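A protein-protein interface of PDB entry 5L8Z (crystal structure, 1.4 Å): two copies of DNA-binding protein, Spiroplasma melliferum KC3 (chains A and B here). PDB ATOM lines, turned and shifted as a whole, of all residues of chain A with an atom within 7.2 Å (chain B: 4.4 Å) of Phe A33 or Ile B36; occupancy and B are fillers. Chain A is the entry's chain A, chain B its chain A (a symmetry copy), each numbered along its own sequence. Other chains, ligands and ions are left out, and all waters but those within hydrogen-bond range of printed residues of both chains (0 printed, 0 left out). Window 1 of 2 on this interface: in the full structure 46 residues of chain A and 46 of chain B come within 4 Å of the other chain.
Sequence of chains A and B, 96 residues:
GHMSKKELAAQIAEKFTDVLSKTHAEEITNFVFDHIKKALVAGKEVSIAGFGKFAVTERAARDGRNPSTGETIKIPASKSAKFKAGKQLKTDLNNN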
ATOM      1  N   MET A   3     -12.837  14.379 -34.125  1.00  0.00           N
ATOM      2  CA  MET A   3     -13.058  15.017 -32.883  1.00  0.00           C
ATOM      3  C   MET A   3     -11.891  14.687 -32.002  1.00  0.00           C
ATOM      4  O   MET A   3     -11.487  13.537 -31.861  1.00  0.00           O
ATOM      5  CB  MET A   3     -14.312  14.493 -32.195  1.00  0.00           C
ATOM      6  CG  MET A   3     -14.458  15.235 -30.856  1.00  0.00           C
ATOM      7  SD  MET A   3     -15.960  14.774 -30.005  1.00  0.00           S
ATOM      8  CE  MET A   3     -15.655  13.081 -29.557  1.00  0.00           C
ATOM      9  N   LYS A   5      -9.524  15.201 -28.245  1.00  0.00           N
ATOM     10  CA  LYS A   5      -9.791  15.317 -26.858  1.00  0.00           C
ATOM     11  C   LYS A   5     -10.184  16.710 -26.422  1.00  0.00           C
ATOM     12  O   LYS A   5     -11.033  16.895 -25.614  1.00  0.00           O
ATOM     13  CB  LYS A   5      -8.579  14.817 -26.096  1.00  0.00           C
ATOM     14  CG  LYS A   5      -8.714  14.867 -24.607  1.00  0.00           C
ATOM     15  CD  LYS A   5      -7.485  14.216 -23.930  1.00  0.00           C
ATOM     16  CE  LYS A   5      -6.233  15.026 -24.294  1.00  0.00           C
ATOM     17  NZ  LYS A   5      -6.474  16.453 -23.902  1.00  0.00           N
ATOM     18  N   LEU A   8     -13.684  17.219 -27.324  1.00  0.00           N
ATOM     19  CA  LEU A   8     -14.521  16.527 -26.384  1.00  0.00           C
ATOM     20  C   LEU A   8     -14.623  17.323 -25.104  1.00  0.00           C
ATOM     21  O   LEU A   8     -15.700  17.483 -24.552  1.00  0.00           O
ATOM     22  CB  LEU A   8     -13.894  15.159 -26.147  1.00  0.00           C
ATOM     23  CG  LEU A   8     -14.585  14.322 -25.095  1.00  0.00           C
ATOM     24  CD1 LEU A   8     -16.022  14.018 -25.467  1.00  0.00           C
ATOM     25  CD2 LEU A   8     -13.766  13.043 -25.026  1.00  0.00           C
ATOM     26  N   ILE A  12     -17.962  18.894 -23.246  1.00  0.00           N
ATOM     27  CA  ILE A  12     -18.294  18.710 -21.848  1.00  0.00           C
ATOM     28  C   ILE A  12     -18.488  20.070 -21.157  1.00  0.00           C
ATOM     29  O   ILE A  12     -19.418  20.277 -20.467  1.00  0.00           O
ATOM     30  CB  ILE A  12     -17.238  17.847 -21.159  1.00  0.00           C
ATOM     31  CG1 ILE A  12     -17.296  16.431 -21.763  1.00  0.00           C
ATOM     32  CG2 ILE A  12     -17.405  17.877 -19.634  1.00  0.00           C
ATOM     33  CD1 ILE A  12     -16.090  15.568 -21.451  1.00  0.00           C
ATOM     34  N   GLU A  27      -9.433  19.123 -17.448  1.00  0.00           N
ATOM     35  CA  GLU A  27      -8.773  18.281 -16.446  1.00  0.00           C
ATOM     36  C   GLU A  27      -9.481  16.986 -16.282  1.00  0.00           C
ATOM     37  O   GLU A  27      -8.882  15.916 -16.235  1.00  0.00           O
ATOM     38  CB  GLU A  27      -8.756  18.970 -15.112  1.00  0.00           C
ATOM     39  CG  GLU A  27      -7.581  18.661 -14.231  1.00  0.00           C
ATOM     40  CD  GLU A  27      -7.520  19.583 -13.040  1.00  0.00           C
ATOM     41  OE1 GLU A  27      -8.175  20.643 -13.058  1.00  0.00           O
ATOM     42  OE2 GLU A  27      -6.767  19.255 -12.106  1.00  0.00           O
ATOM     43  N   ILE A  28     -10.777  16.982 -16.218  1.00  0.00           N
ATOM     44  CA  ILE A  28     -11.474  15.777 -15.985  1.00  0.00           C
ATOM     45  C   ILE A  28     -11.414  14.917 -17.197  1.00  0.00           C
ATOM     46  O   ILE A  28     -11.280  13.676 -17.077  1.00  0.00           O
ATOM     47  CB  ILE A  28     -12.905  16.099 -15.586  1.00  0.00           C
ATOM     48  CG1 ILE A  28     -12.751  16.623 -14.167  1.00  0.00           C
ATOM     49  CG2 ILE A  28     -13.809  14.891 -15.591  1.00  0.00           C
ATOM     50  CD1 ILE A  28     -14.003  17.191 -13.587  1.00  0.00           C
ATOM     51  N   THR A  29     -11.541  15.488 -18.391  1.00  0.00           N
ATOM     52  CA  THR A  29     -11.435  14.676 -19.588  1.00  0.00           C
ATOM     53  C   THR A  29     -10.076  14.023 -19.620  1.00  0.00           C
ATOM     54  O   THR A  29      -9.983  12.834 -19.946  1.00  0.00           O
ATOM     55  CB  THR A  29     -11.649  15.554 -20.797  1.00  0.00           C
ATOM     56  OG1 THR A  29     -12.927  16.162 -20.758  1.00  0.00           O
ATOM     57  CG2 THR A  29     -11.553  14.742 -22.098  1.00  0.00           C
ATOM     58  N   ASN A  30      -9.023  14.758 -19.294  1.00  0.00           N
ATOM     59  CA  ASN A  30      -7.697  14.137 -19.282  1.00  0.00           C
ATOM     60  C   ASN A  30      -7.678  13.061 -18.234  1.00  0.00           C
ATOM     61  O   ASN A  30      -7.119  11.967 -18.462  1.00  0.00           O
ATOM     62  CB  ASN A  30      -6.628  15.139 -18.913  1.00  0.00           C
ATOM     63  CG  ASN A  30      -6.335  16.127 -20.027  1.00  0.00           C
ATOM     64  OD1 ASN A  30      -6.640  15.880 -21.160  1.00  0.00           O
ATOM     65  ND2 ASN A  30      -5.794  17.255 -19.671  1.00  0.00           N
ATOM     66  N   PHE A  31      -8.348  13.279 -17.106  1.00  0.00           N
ATOM     67  CA  PHE A  31      -8.303  12.260 -16.059  1.00  0.00           C
ATOM     68  C   PHE A  31      -9.033  11.007 -16.495  1.00  0.00           C
ATOM     69  O   PHE A  31      -8.563   9.918 -16.178  1.00  0.00           O
ATOM     70  CB  PHE A  31      -8.948  12.832 -14.793  1.00  0.00           C
ATOM     71  CG  PHE A  31      -8.840  11.904 -13.638  1.00  0.00           C
ATOM     72  CD1 PHE A  31      -9.783  10.921 -13.461  1.00  0.00           C
ATOM     73  CD2 PHE A  31      -7.767  11.986 -12.824  1.00  0.00           C
ATOM     74  CE1 PHE A  31      -9.708  10.029 -12.389  1.00  0.00           C
ATOM     75  CE2 PHE A  31      -7.654  11.108 -11.743  1.00  0.00           C
ATOM     76  CZ  PHE A  31      -8.585  10.110 -11.544  1.00  0.00           C
ATOM     77  N   VAL A  32     -10.130  11.102 -17.217  1.00  0.00           N
ATOM     78  CA  VAL A  32     -10.810   9.943 -17.683  1.00  0.00           C
ATOM     79  C   VAL A  32      -9.838   9.000 -18.372  1.00  0.00           C
ATOM     80  O   VAL A  32      -9.751   7.820 -18.028  1.00  0.00           O
ATOM     81  CB  VAL A  32     -11.904  10.352 -18.657  1.00  0.00           C
ATOM     82  CG1 VAL A  32     -12.397   9.130 -19.401  1.00  0.00           C
ATOM     83  CG2 VAL A  32     -13.045  11.008 -17.883  1.00  0.00           C
ATOM     84  N   PHE A  33      -9.073   9.536 -19.318  1.00  0.00           N
ATOM     85  CA  PHE A  33      -8.252   8.667 -20.129  1.00  0.00           C
ATOM     86  C   PHE A  33      -7.003   8.295 -19.388  1.00  0.00           C
ATOM     87  O   PHE A  33      -6.550   7.175 -19.512  1.00  0.00           O
ATOM     88  CB  PHE A  33      -7.974   9.312 -21.481  1.00  0.00           C
ATOM     89  CG  PHE A  33      -9.194   9.464 -22.243  1.00  0.00           C
ATOM     90  CD1 PHE A  33      -9.745   8.365 -22.811  1.00  0.00           C
ATOM     91  CD2 PHE A  33      -9.860  10.668 -22.249  1.00  0.00           C
ATOM     92  CE1 PHE A  33     -10.952   8.450 -23.487  1.00  0.00           C
ATOM     93  CE2 PHE A  33     -11.065  10.781 -22.899  1.00  0.00           C
ATOM     94  CZ  PHE A  33     -11.617   9.667 -23.509  1.00  0.00           C
ATOM     95  N   ASP A  34      -6.530   9.169 -18.517  1.00  0.00           N
ATOM     96  CA  ASP A  34      -5.374   8.782 -17.736  1.00  0.00           C
ATOM     97  C   ASP A  34      -5.755   7.671 -16.826  1.00  0.00           C
ATOM     98  O   ASP A  34      -4.957   6.792 -16.592  1.00  0.00           O
ATOM     99  CB  ASP A  34      -4.873   9.988 -16.920  1.00  0.00           C
ATOM    100  CG  ASP A  34      -4.174  11.018 -17.751  1.00  0.00           C
ATOM    101  OD1 ASP A  34      -3.857  10.824 -18.956  1.00  0.00           O
ATOM    102  OD2 ASP A  34      -3.928  12.059 -17.114  1.00  0.00           O
ATOM    103  N   HIS A  35      -6.945   7.713 -16.246  1.00  0.00           N
ATOM    104  CA  HIS A  35      -7.309   6.737 -15.317  1.00  0.00           C
ATOM    105  C   HIS A  35      -7.554   5.396 -16.024  1.00  0.00           C
ATOM    106  O   HIS A  35      -7.194   4.382 -15.510  1.00  0.00           O
ATOM    107  CB  HIS A  35      -8.461   7.156 -14.493  1.00  0.00           C
ATOM    108  CG  HIS A  35      -8.577   6.323 -13.312  1.00  0.00           C
ATOM    109  ND1 HIS A  35      -7.608   6.369 -12.333  1.00  0.00           N
ATOM    110  CD2 HIS A  35      -9.534   5.452 -12.906  1.00  0.00           C
ATOM    111  CE1 HIS A  35      -7.975   5.528 -11.392  1.00  0.00           C
ATOM    112  NE2 HIS A  35      -9.114   4.956 -11.708  1.00  0.00           N
ATOM    113  N   ILE A  36      -8.135   5.428 -17.204  1.00  0.00           N
ATOM    114  CA  ILE A  36      -8.307   4.249 -17.990  1.00  0.00           C
ATOM    115  C   ILE A  36      -6.924   3.671 -18.335  1.00  0.00           C
ATOM    116  O   ILE A  36      -6.688   2.509 -18.163  1.00  0.00           O
ATOM    117  CB  ILE A  36      -9.113   4.507 -19.240  1.00  0.00           C
ATOM    118  CG1 ILE A  36     -10.553   4.840 -18.820  1.00  0.00           C
ATOM    119  CG2 ILE A  36      -9.030   3.325 -20.208  1.00  0.00           C
ATOM    120  CD1 ILE A  36     -11.421   5.300 -19.972  1.00  0.00           C
ATOM    121  N   LYS A  37      -5.988   4.507 -18.777  1.00  0.00           N
ATOM    122  CA  LYS A  37      -4.672   4.015 -18.976  1.00  0.00           C
ATOM    123  C   LYS A  37      -4.091   3.436 -17.719  1.00  0.00           C
ATOM    124  O   LYS A  37      -3.447   2.390 -17.828  1.00  0.00           O
ATOM    125  CB  LYS A  37      -3.821   5.155 -19.442  1.00  0.00           C
ATOM    126  CG  LYS A  37      -4.123   5.588 -20.860  1.00  0.00           C
ATOM    127  CD  LYS A  37      -3.072   6.439 -21.532  1.00  0.00           C
ATOM    128  CE  LYS A  37      -2.964   7.790 -20.898  1.00  0.00           C
ATOM    129  NZ  LYS A  37      -1.747   8.443 -21.460  1.00  0.00           N
ATOM    130  N   LYS A  38      -4.234   4.095 -16.596  1.00  0.00           N
ATOM    131  CA  LYS A  38      -3.653   3.537 -15.367  1.00  0.00           C
ATOM    132  C   LYS A  38      -4.239   2.181 -15.120  1.00  0.00           C
ATOM    133  O   LYS A  38      -3.490   1.245 -14.743  1.00  0.00           O
ATOM    134  CB  LYS A  38      -3.883   4.522 -14.214  1.00  0.00           C
ATOM    135  CG  LYS A  38      -2.798   5.609 -14.360  1.00  0.00           C
ATOM    136  CD  LYS A  38      -2.878   6.627 -13.224  1.00  0.00           C
ATOM    137  N   ALA A  39      -5.519   2.008 -15.285  1.00  0.00           N
ATOM    138  CA  ALA A  39      -6.122   0.711 -15.105  1.00  0.00           C
ATOM    139  C   ALA A  39      -5.596  -0.325 -16.063  1.00  0.00           C
ATOM    140  O   ALA A  39      -5.265  -1.418 -15.600  1.00  0.00           O
ATOM    141  CB  ALA A  39      -7.619   0.840 -15.253  1.00  0.00           C
ATOM    142  N   LEU A  40      -5.388   0.009 -17.345  1.00  0.00           N
ATOM    143  CA  LEU A  40      -4.801  -0.969 -18.246  1.00  0.00           C
ATOM    144  C   LEU A  40      -3.403  -1.290 -17.869  1.00  0.00           C
ATOM    145  O   LEU A  40      -3.003  -2.450 -17.903  1.00  0.00           O
ATOM    146  CB  LEU A  40      -4.848  -0.359 -19.644  1.00  0.00           C
ATOM    147  CG  LEU A  40      -6.259  -0.207 -20.195  1.00  0.00           C
ATOM    148  CD1 LEU A  40      -6.207   0.695 -21.381  1.00  0.00           C
ATOM    149  CD2 LEU A  40      -6.906  -1.570 -20.525  1.00  0.00           C
ATOM    150  N   PHE A  51     -20.495   1.281 -24.243  1.00  0.00           N
ATOM    151  CA  PHE A  51     -19.428   1.774 -25.121  1.00  0.00           C
ATOM    152  C   PHE A  51     -18.586   0.619 -25.615  1.00  0.00           C
ATOM    153  O   PHE A  51     -18.553   0.253 -26.776  1.00  0.00           O
ATOM    154  CB  PHE A  51     -18.569   2.788 -24.396  1.00  0.00           C
ATOM    155  CG  PHE A  51     -17.583   3.475 -25.278  1.00  0.00           C
ATOM    156  CD1 PHE A  51     -17.973   4.312 -26.331  1.00  0.00           C
ATOM    157  CD2 PHE A  51     -16.249   3.156 -25.148  1.00  0.00           C
ATOM    158  CE1 PHE A  51     -17.019   4.943 -27.134  1.00  0.00           C
ATOM    159  CE2 PHE A  51     -15.300   3.775 -25.951  1.00  0.00           C
ATOM    160  CZ  PHE A  51     -15.682   4.658 -26.935  1.00  0.00           C
ATOM    161  N   PHE A  54     -11.893  -2.242 -22.930  1.00  0.00           N
ATOM    162  CA  PHE A  54     -10.460  -2.188 -23.241  1.00  0.00           C
ATOM    163  C   PHE A  54      -9.791  -3.247 -22.457  1.00  0.00           C
ATOM    164  O   PHE A  54      -9.995  -3.409 -21.304  1.00  0.00           O
ATOM    165  CB  PHE A  54      -9.868  -0.836 -22.832  1.00  0.00           C
ATOM    166  CG  PHE A  54     -10.559   0.350 -23.462  1.00  0.00           C
ATOM    167  CD1 PHE A  54     -11.677   0.888 -22.881  1.00  0.00           C
ATOM    168  CD2 PHE A  54     -10.005   0.964 -24.618  1.00  0.00           C
ATOM    169  CE1 PHE A  54     -12.292   1.969 -23.496  1.00  0.00           C
ATOM    170  CE2 PHE A  54     -10.613   2.034 -25.170  1.00  0.00           C
ATOM    171  CZ  PHE A  54     -11.704   2.581 -24.622  1.00  0.00           C
ATOM    172  N   LEU A  89     -22.865   0.291 -29.070  1.00  0.00           N
ATOM    173  CA  LEU A  89     -22.139   1.038 -30.056  1.00  0.00           C
ATOM    174  C   LEU A  89     -22.271   0.394 -31.430  1.00  0.00           C
ATOM    175  O   LEU A  89     -22.503   1.079 -32.418  1.00  0.00           O
ATOM    176  CB  LEU A  89     -20.692   1.109 -29.619  1.00  0.00           C
ATOM    177  CG  LEU A  89     -19.764   1.829 -30.604  1.00  0.00           C
ATOM    178  CD1 LEU A  89     -20.308   3.238 -30.950  1.00  0.00           C
ATOM    179  CD2 LEU A  89     -18.441   1.881 -29.826  1.00  0.00           C
ATOM    180  N   VAL B  32     -18.937  11.593 -21.621  1.00  0.00           N
ATOM    181  CA  VAL B  32     -17.736  11.372 -22.351  1.00  0.00           C
ATOM    182  C   VAL B  32     -17.947  10.300 -23.408  1.00  0.00           C
ATOM    183  O   VAL B  32     -17.669  10.514 -24.588  1.00  0.00           O
ATOM    184  CB  VAL B  32     -16.633  10.940 -21.396  1.00  0.00           C
ATOM    185  CG1 VAL B  32     -15.470  10.387 -22.191  1.00  0.00           C
ATOM    186  CG2 VAL B  32     -16.193  12.140 -20.562  1.00  0.00           C
ATOM    187  N   PHE B  33     -18.484   9.159 -22.986  1.00  0.00           N
ATOM    188  CA  PHE B  33     -18.554   8.041 -23.896  1.00  0.00           C
ATOM    189  C   PHE B  33     -19.723   8.200 -24.822  1.00  0.00           C
ATOM    190  O   PHE B  33     -19.618   7.842 -25.977  1.00  0.00           O
ATOM    191  CB  PHE B  33     -18.581   6.729 -23.123  1.00  0.00           C
ATOM    192  CG  PHE B  33     -17.341   6.527 -22.403  1.00  0.00           C
ATOM    193  CD1 PHE B  33     -16.239   6.164 -23.102  1.00  0.00           C
ATOM    194  CD2 PHE B  33     -17.254   6.855 -21.070  1.00  0.00           C
ATOM    195  CE1 PHE B  33     -15.014   6.032 -22.466  1.00  0.00           C
ATOM    196  CE2 PHE B  33     -16.050   6.747 -20.416  1.00  0.00           C
ATOM    197  CZ  PHE B  33     -14.927   6.346 -21.119  1.00  0.00           C
ATOM    198  N   ASP B  34     -20.774   8.858 -24.366  1.00  0.00           N
ATOM    199  CA  ASP B  34     -21.871   9.090 -25.281  1.00  0.00           C
ATOM    200  C   ASP B  34     -21.419  10.012 -26.355  1.00  0.00           C
ATOM    201  O   ASP B  34     -21.828   9.858 -27.484  1.00  0.00           O
ATOM    202  CB  ASP B  34     -23.060   9.705 -24.519  1.00  0.00           C
ATOM    203  CG  ASP B  34     -23.777   8.723 -23.646  1.00  0.00           C
ATOM    204  OD1 ASP B  34     -23.553   7.483 -23.684  1.00  0.00           O
ATOM    205  OD2 ASP B  34     -24.622   9.267 -22.910  1.00  0.00           O
ATOM    206  N   HIS B  35     -20.626  11.020 -26.025  1.00  0.00           N
ATOM    207  CA  HIS B  35     -20.248  11.960 -26.985  1.00  0.00           C
ATOM    208  C   HIS B  35     -19.261  11.335 -27.981  1.00  0.00           C
ATOM    209  O   HIS B  35     -19.340  11.605 -29.140  1.00  0.00           O
ATOM    210  CB  HIS B  35     -19.722  13.197 -26.374  1.00  0.00           C
ATOM    211  CG  HIS B  35     -19.699  14.278 -27.341  1.00  0.00           C
ATOM    212  ND1 HIS B  35     -20.879  14.790 -27.837  1.00  0.00           N
ATOM    213  CD2 HIS B  35     -18.679  14.982 -27.891  1.00  0.00           C
ATOM    214  CE1 HIS B  35     -20.557  15.750 -28.674  1.00  0.00           C
ATOM    215  NE2 HIS B  35     -19.252  15.883 -28.738  1.00  0.00           N
ATOM    216  N   ILE B  36     -18.372  10.488 -27.507  1.00  0.00           N
ATOM    217  CA  ILE B  36     -17.484   9.772 -28.364  1.00  0.00           C
ATOM    218  C   ILE B  36     -18.310   8.871 -29.300  1.00  0.00           C
ATOM    219  O   ILE B  36     -18.106   8.869 -30.480  1.00  0.00           O
ATOM    220  CB  ILE B  36     -16.471   8.964 -27.590  1.00  0.00           C
ATOM    221  CG1 ILE B  36     -15.526   9.941 -26.875  1.00  0.00           C
ATOM    222  CG2 ILE B  36     -15.735   7.977 -28.500  1.00  0.00           C
ATOM    223  CD1 ILE B  36     -14.574   9.259 -25.915  1.00  0.00           C
ATOM    224  N   LYS B  37     -19.285   8.141 -28.766  1.00  0.00           N
ATOM    225  CA  LYS B  37     -20.138   7.405 -29.631  1.00  0.00           C
ATOM    226  C   LYS B  37     -20.834   8.292 -30.620  1.00  0.00           C
ATOM    227  O   LYS B  37     -20.927   7.876 -31.779  1.00  0.00           O
ATOM    228  CB  LYS B  37     -21.154   6.704 -28.784  1.00  0.00           C
ATOM    229  CG  LYS B  37     -20.581   5.551 -27.990  1.00  0.00           C
ATOM    230  CD  LYS B  37     -21.581   4.565 -27.435  1.00  0.00           C
ATOM    231  CE  LYS B  37     -22.430   5.178 -26.368  1.00  0.00           C
ATOM    232  NZ  LYS B  37     -23.530   4.216 -26.074  1.00  0.00           N
ATOM    233  N   LYS B  38     -21.364   9.414 -30.201  1.00  0.00           N
ATOM    234  CA  LYS B  38     -22.060  10.276 -31.167  1.00  0.00           C
ATOM    235  C   LYS B  38     -21.107  10.659 -32.256  1.00  0.00           C
ATOM    236  O   LYS B  38     -21.500  10.652 -33.451  1.00  0.00           O
ATOM    237  CB  LYS B  38     -22.656  11.478 -30.424  1.00  0.00           C
ATOM    238  CG  LYS B  38     -23.960  10.973 -29.775  1.00  0.00           C
ATOM    239  CD  LYS B  38     -24.691  12.101 -29.050  1.00  0.00           C
ATOM    240  N   ALA B  39     -19.893  11.009 -31.938  1.00  0.00           N
ATOM    241  CA  ALA B  39     -18.926  11.341 -32.954  1.00  0.00           C
ATOM    242  C   ALA B  39     -18.629  10.196 -33.886  1.00  0.00           C
ATOM    243  O   ALA B  39     -18.634  10.425 -35.097  1.00  0.00           O
ATOM    244  CB  ALA B  39     -17.655  11.809 -32.288  1.00  0.00           C
ATOM    245  N   LEU B  40     -18.495   8.958 -33.387  1.00  0.00           N
ATOM    246  CA  LEU B  40     -18.292   7.844 -34.298  1.00  0.00           C
ATOM    247  C   LEU B  40     -19.482   7.613 -35.153  1.00  0.00           C
ATOM    248  O   LEU B  40     -19.347   7.357 -36.347  1.00  0.00           O
ATOM    249  CB  LEU B  40     -18.012   6.618 -33.435  1.00  0.00           C
ATOM    250  CG  LEU B  40     -16.684   6.684 -32.693  1.00  0.00           C
ATOM    251  CD1 LEU B  40     -16.679   5.629 -31.641  1.00  0.00           C
ATOM    252  CD2 LEU B  40     -15.477   6.563 -33.649  1.00  0.00           C
ATOM    253  N   VAL B  46     -12.211   9.737 -33.630  1.00  0.00           N
ATOM    254  CA  VAL B  46     -12.043  10.407 -32.379  1.00  0.00           C
ATOM    255  C   VAL B  46     -10.637  10.156 -31.915  1.00  0.00           C
ATOM    256  O   VAL B  46     -10.249   9.037 -31.670  1.00  0.00           O
ATOM    257  CB  VAL B  46     -13.044   9.820 -31.375  1.00  0.00           C
ATOM    258  CG1 VAL B  46     -12.842  10.525 -30.043  1.00  0.00           C
ATOM    259  CG2 VAL B  46     -14.447  10.140 -31.841  1.00  0.00           C
ATOM    260  N   ILE B  48      -7.776  10.807 -29.139  1.00  0.00           N
ATOM    261  CA  ILE B  48      -7.615  11.236 -27.792  1.00  0.00           C
ATOM    262  C   ILE B  48      -6.115  11.203 -27.510  1.00  0.00           C
ATOM    263  O   ILE B  48      -5.495  10.124 -27.368  1.00  0.00           O
ATOM    264  CB  ILE B  48      -8.340  10.277 -26.832  1.00  0.00           C
ATOM    265  CG1 ILE B  48      -9.830  10.142 -27.119  1.00  0.00           C
ATOM    266  CG2 ILE B  48      -8.124  10.665 -25.390  1.00  0.00           C
ATOM    267  CD1 ILE B  48     -10.639  11.439 -26.951  1.00  0.00           C
ATOM    268  N   PHE B  51      -3.787   8.743 -25.573  1.00  0.00           N
ATOM    269  CA  PHE B  51      -4.587   7.541 -25.309  1.00  0.00           C
ATOM    270  C   PHE B  51      -4.671   6.688 -26.555  1.00  0.00           C
ATOM    271  O   PHE B  51      -4.151   5.591 -26.662  1.00  0.00           O
ATOM    272  CB  PHE B  51      -5.972   7.919 -24.828  1.00  0.00           C
ATOM    273  CG  PHE B  51      -6.778   6.758 -24.358  1.00  0.00           C
ATOM    274  CD1 PHE B  51      -6.417   5.996 -23.239  1.00  0.00           C
ATOM    275  CD2 PHE B  51      -7.829   6.326 -25.138  1.00  0.00           C
ATOM    276  CE1 PHE B  51      -7.201   4.916 -22.825  1.00  0.00           C
ATOM    277  CE2 PHE B  51      -8.605   5.248 -24.732  1.00  0.00           C
ATOM    278  CZ  PHE B  51      -8.292   4.549 -23.589  1.00  0.00           C
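Phe A33 touches Ile B36, and with the chains exchanged Ile A36 touches Phe B33. Phe A33 touches Phe B51, and with the chains exchanged Phe A51 touches Phe B33. Ile A36 touches Phe B51, and with the chains exchanged Phe A51 touches Ile B36. Lys A37 touches Phe B51, and with the chains exchanged Phe A51 touches Lys B37. Positions printed for both chains: 32, 33, 34, 35, 36, 37, 38, 39, 40 and 51. Of the 20 pairs that touch across the chains among the printed residues, 8 have their exchanged pair printed and touching as well.
Hydrophobic or aromatic side chains of chain B that line the printed part of chain A: Val B32, Phe B33, His B35, Ile B36, Ala B39, Val B46, Ile B48 and Phe B51.
A ring nitrogen (NE2) of His B35 lies close to the side-chain sulfur (SD) of Met A3.
Ile B36 touches Met A3. Met A3 touches Val B46. Lys A5 touches Ile B48. O of Val B32 touches CD1 of Leu A8 (3.97 Å). CD1 of Leu A8 touches CD2 of His B35 (3.7 Å). CD1 of Ile A36 touches CZ of Phe B33 (3.8 Å). Phe B51 touches Ile A36 (CE1 to CG2, 3.6 Å). Lys A37 touches Phe B51. Phe A51 touches Ile B36. Phe A54 touches Phe B51.
Of the printed residues of chain B, Met A3 touches His B35, Ile B36, Ala B39 and Val B46. Of the printed residues of chain B, Ile A12 touches Val B32. Phe A33 touches three residues of chain B. Of the printed residues of chain B, Ile A36 touches Phe B33 (3.8 Å) and Phe B51 (3.6 Å). Of the printed residues of chain A, Val B32 touches Leu A8 (3.97 Å) and Ile A12 (3.5 Å). Printed residues of chain A within 4 Å of Phe B33: Ile A36 and Phe A51. Ile B36 touches just these residues of chain A: Met A3, Leu A8, Phe A33 and Phe A51. The nearest residue of chain B that does not touch Phe A33 is Val B32 (4.1 Å). The nearest residue of chain A that does not touch Ile B36 is Leu A89 (6.1 Å).
The side-chain amino group (NZ) of Lys A5 is in hydrogen-bond range of the side-chain amide oxygen (OD1) of Asn A30 (2.8 Å).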
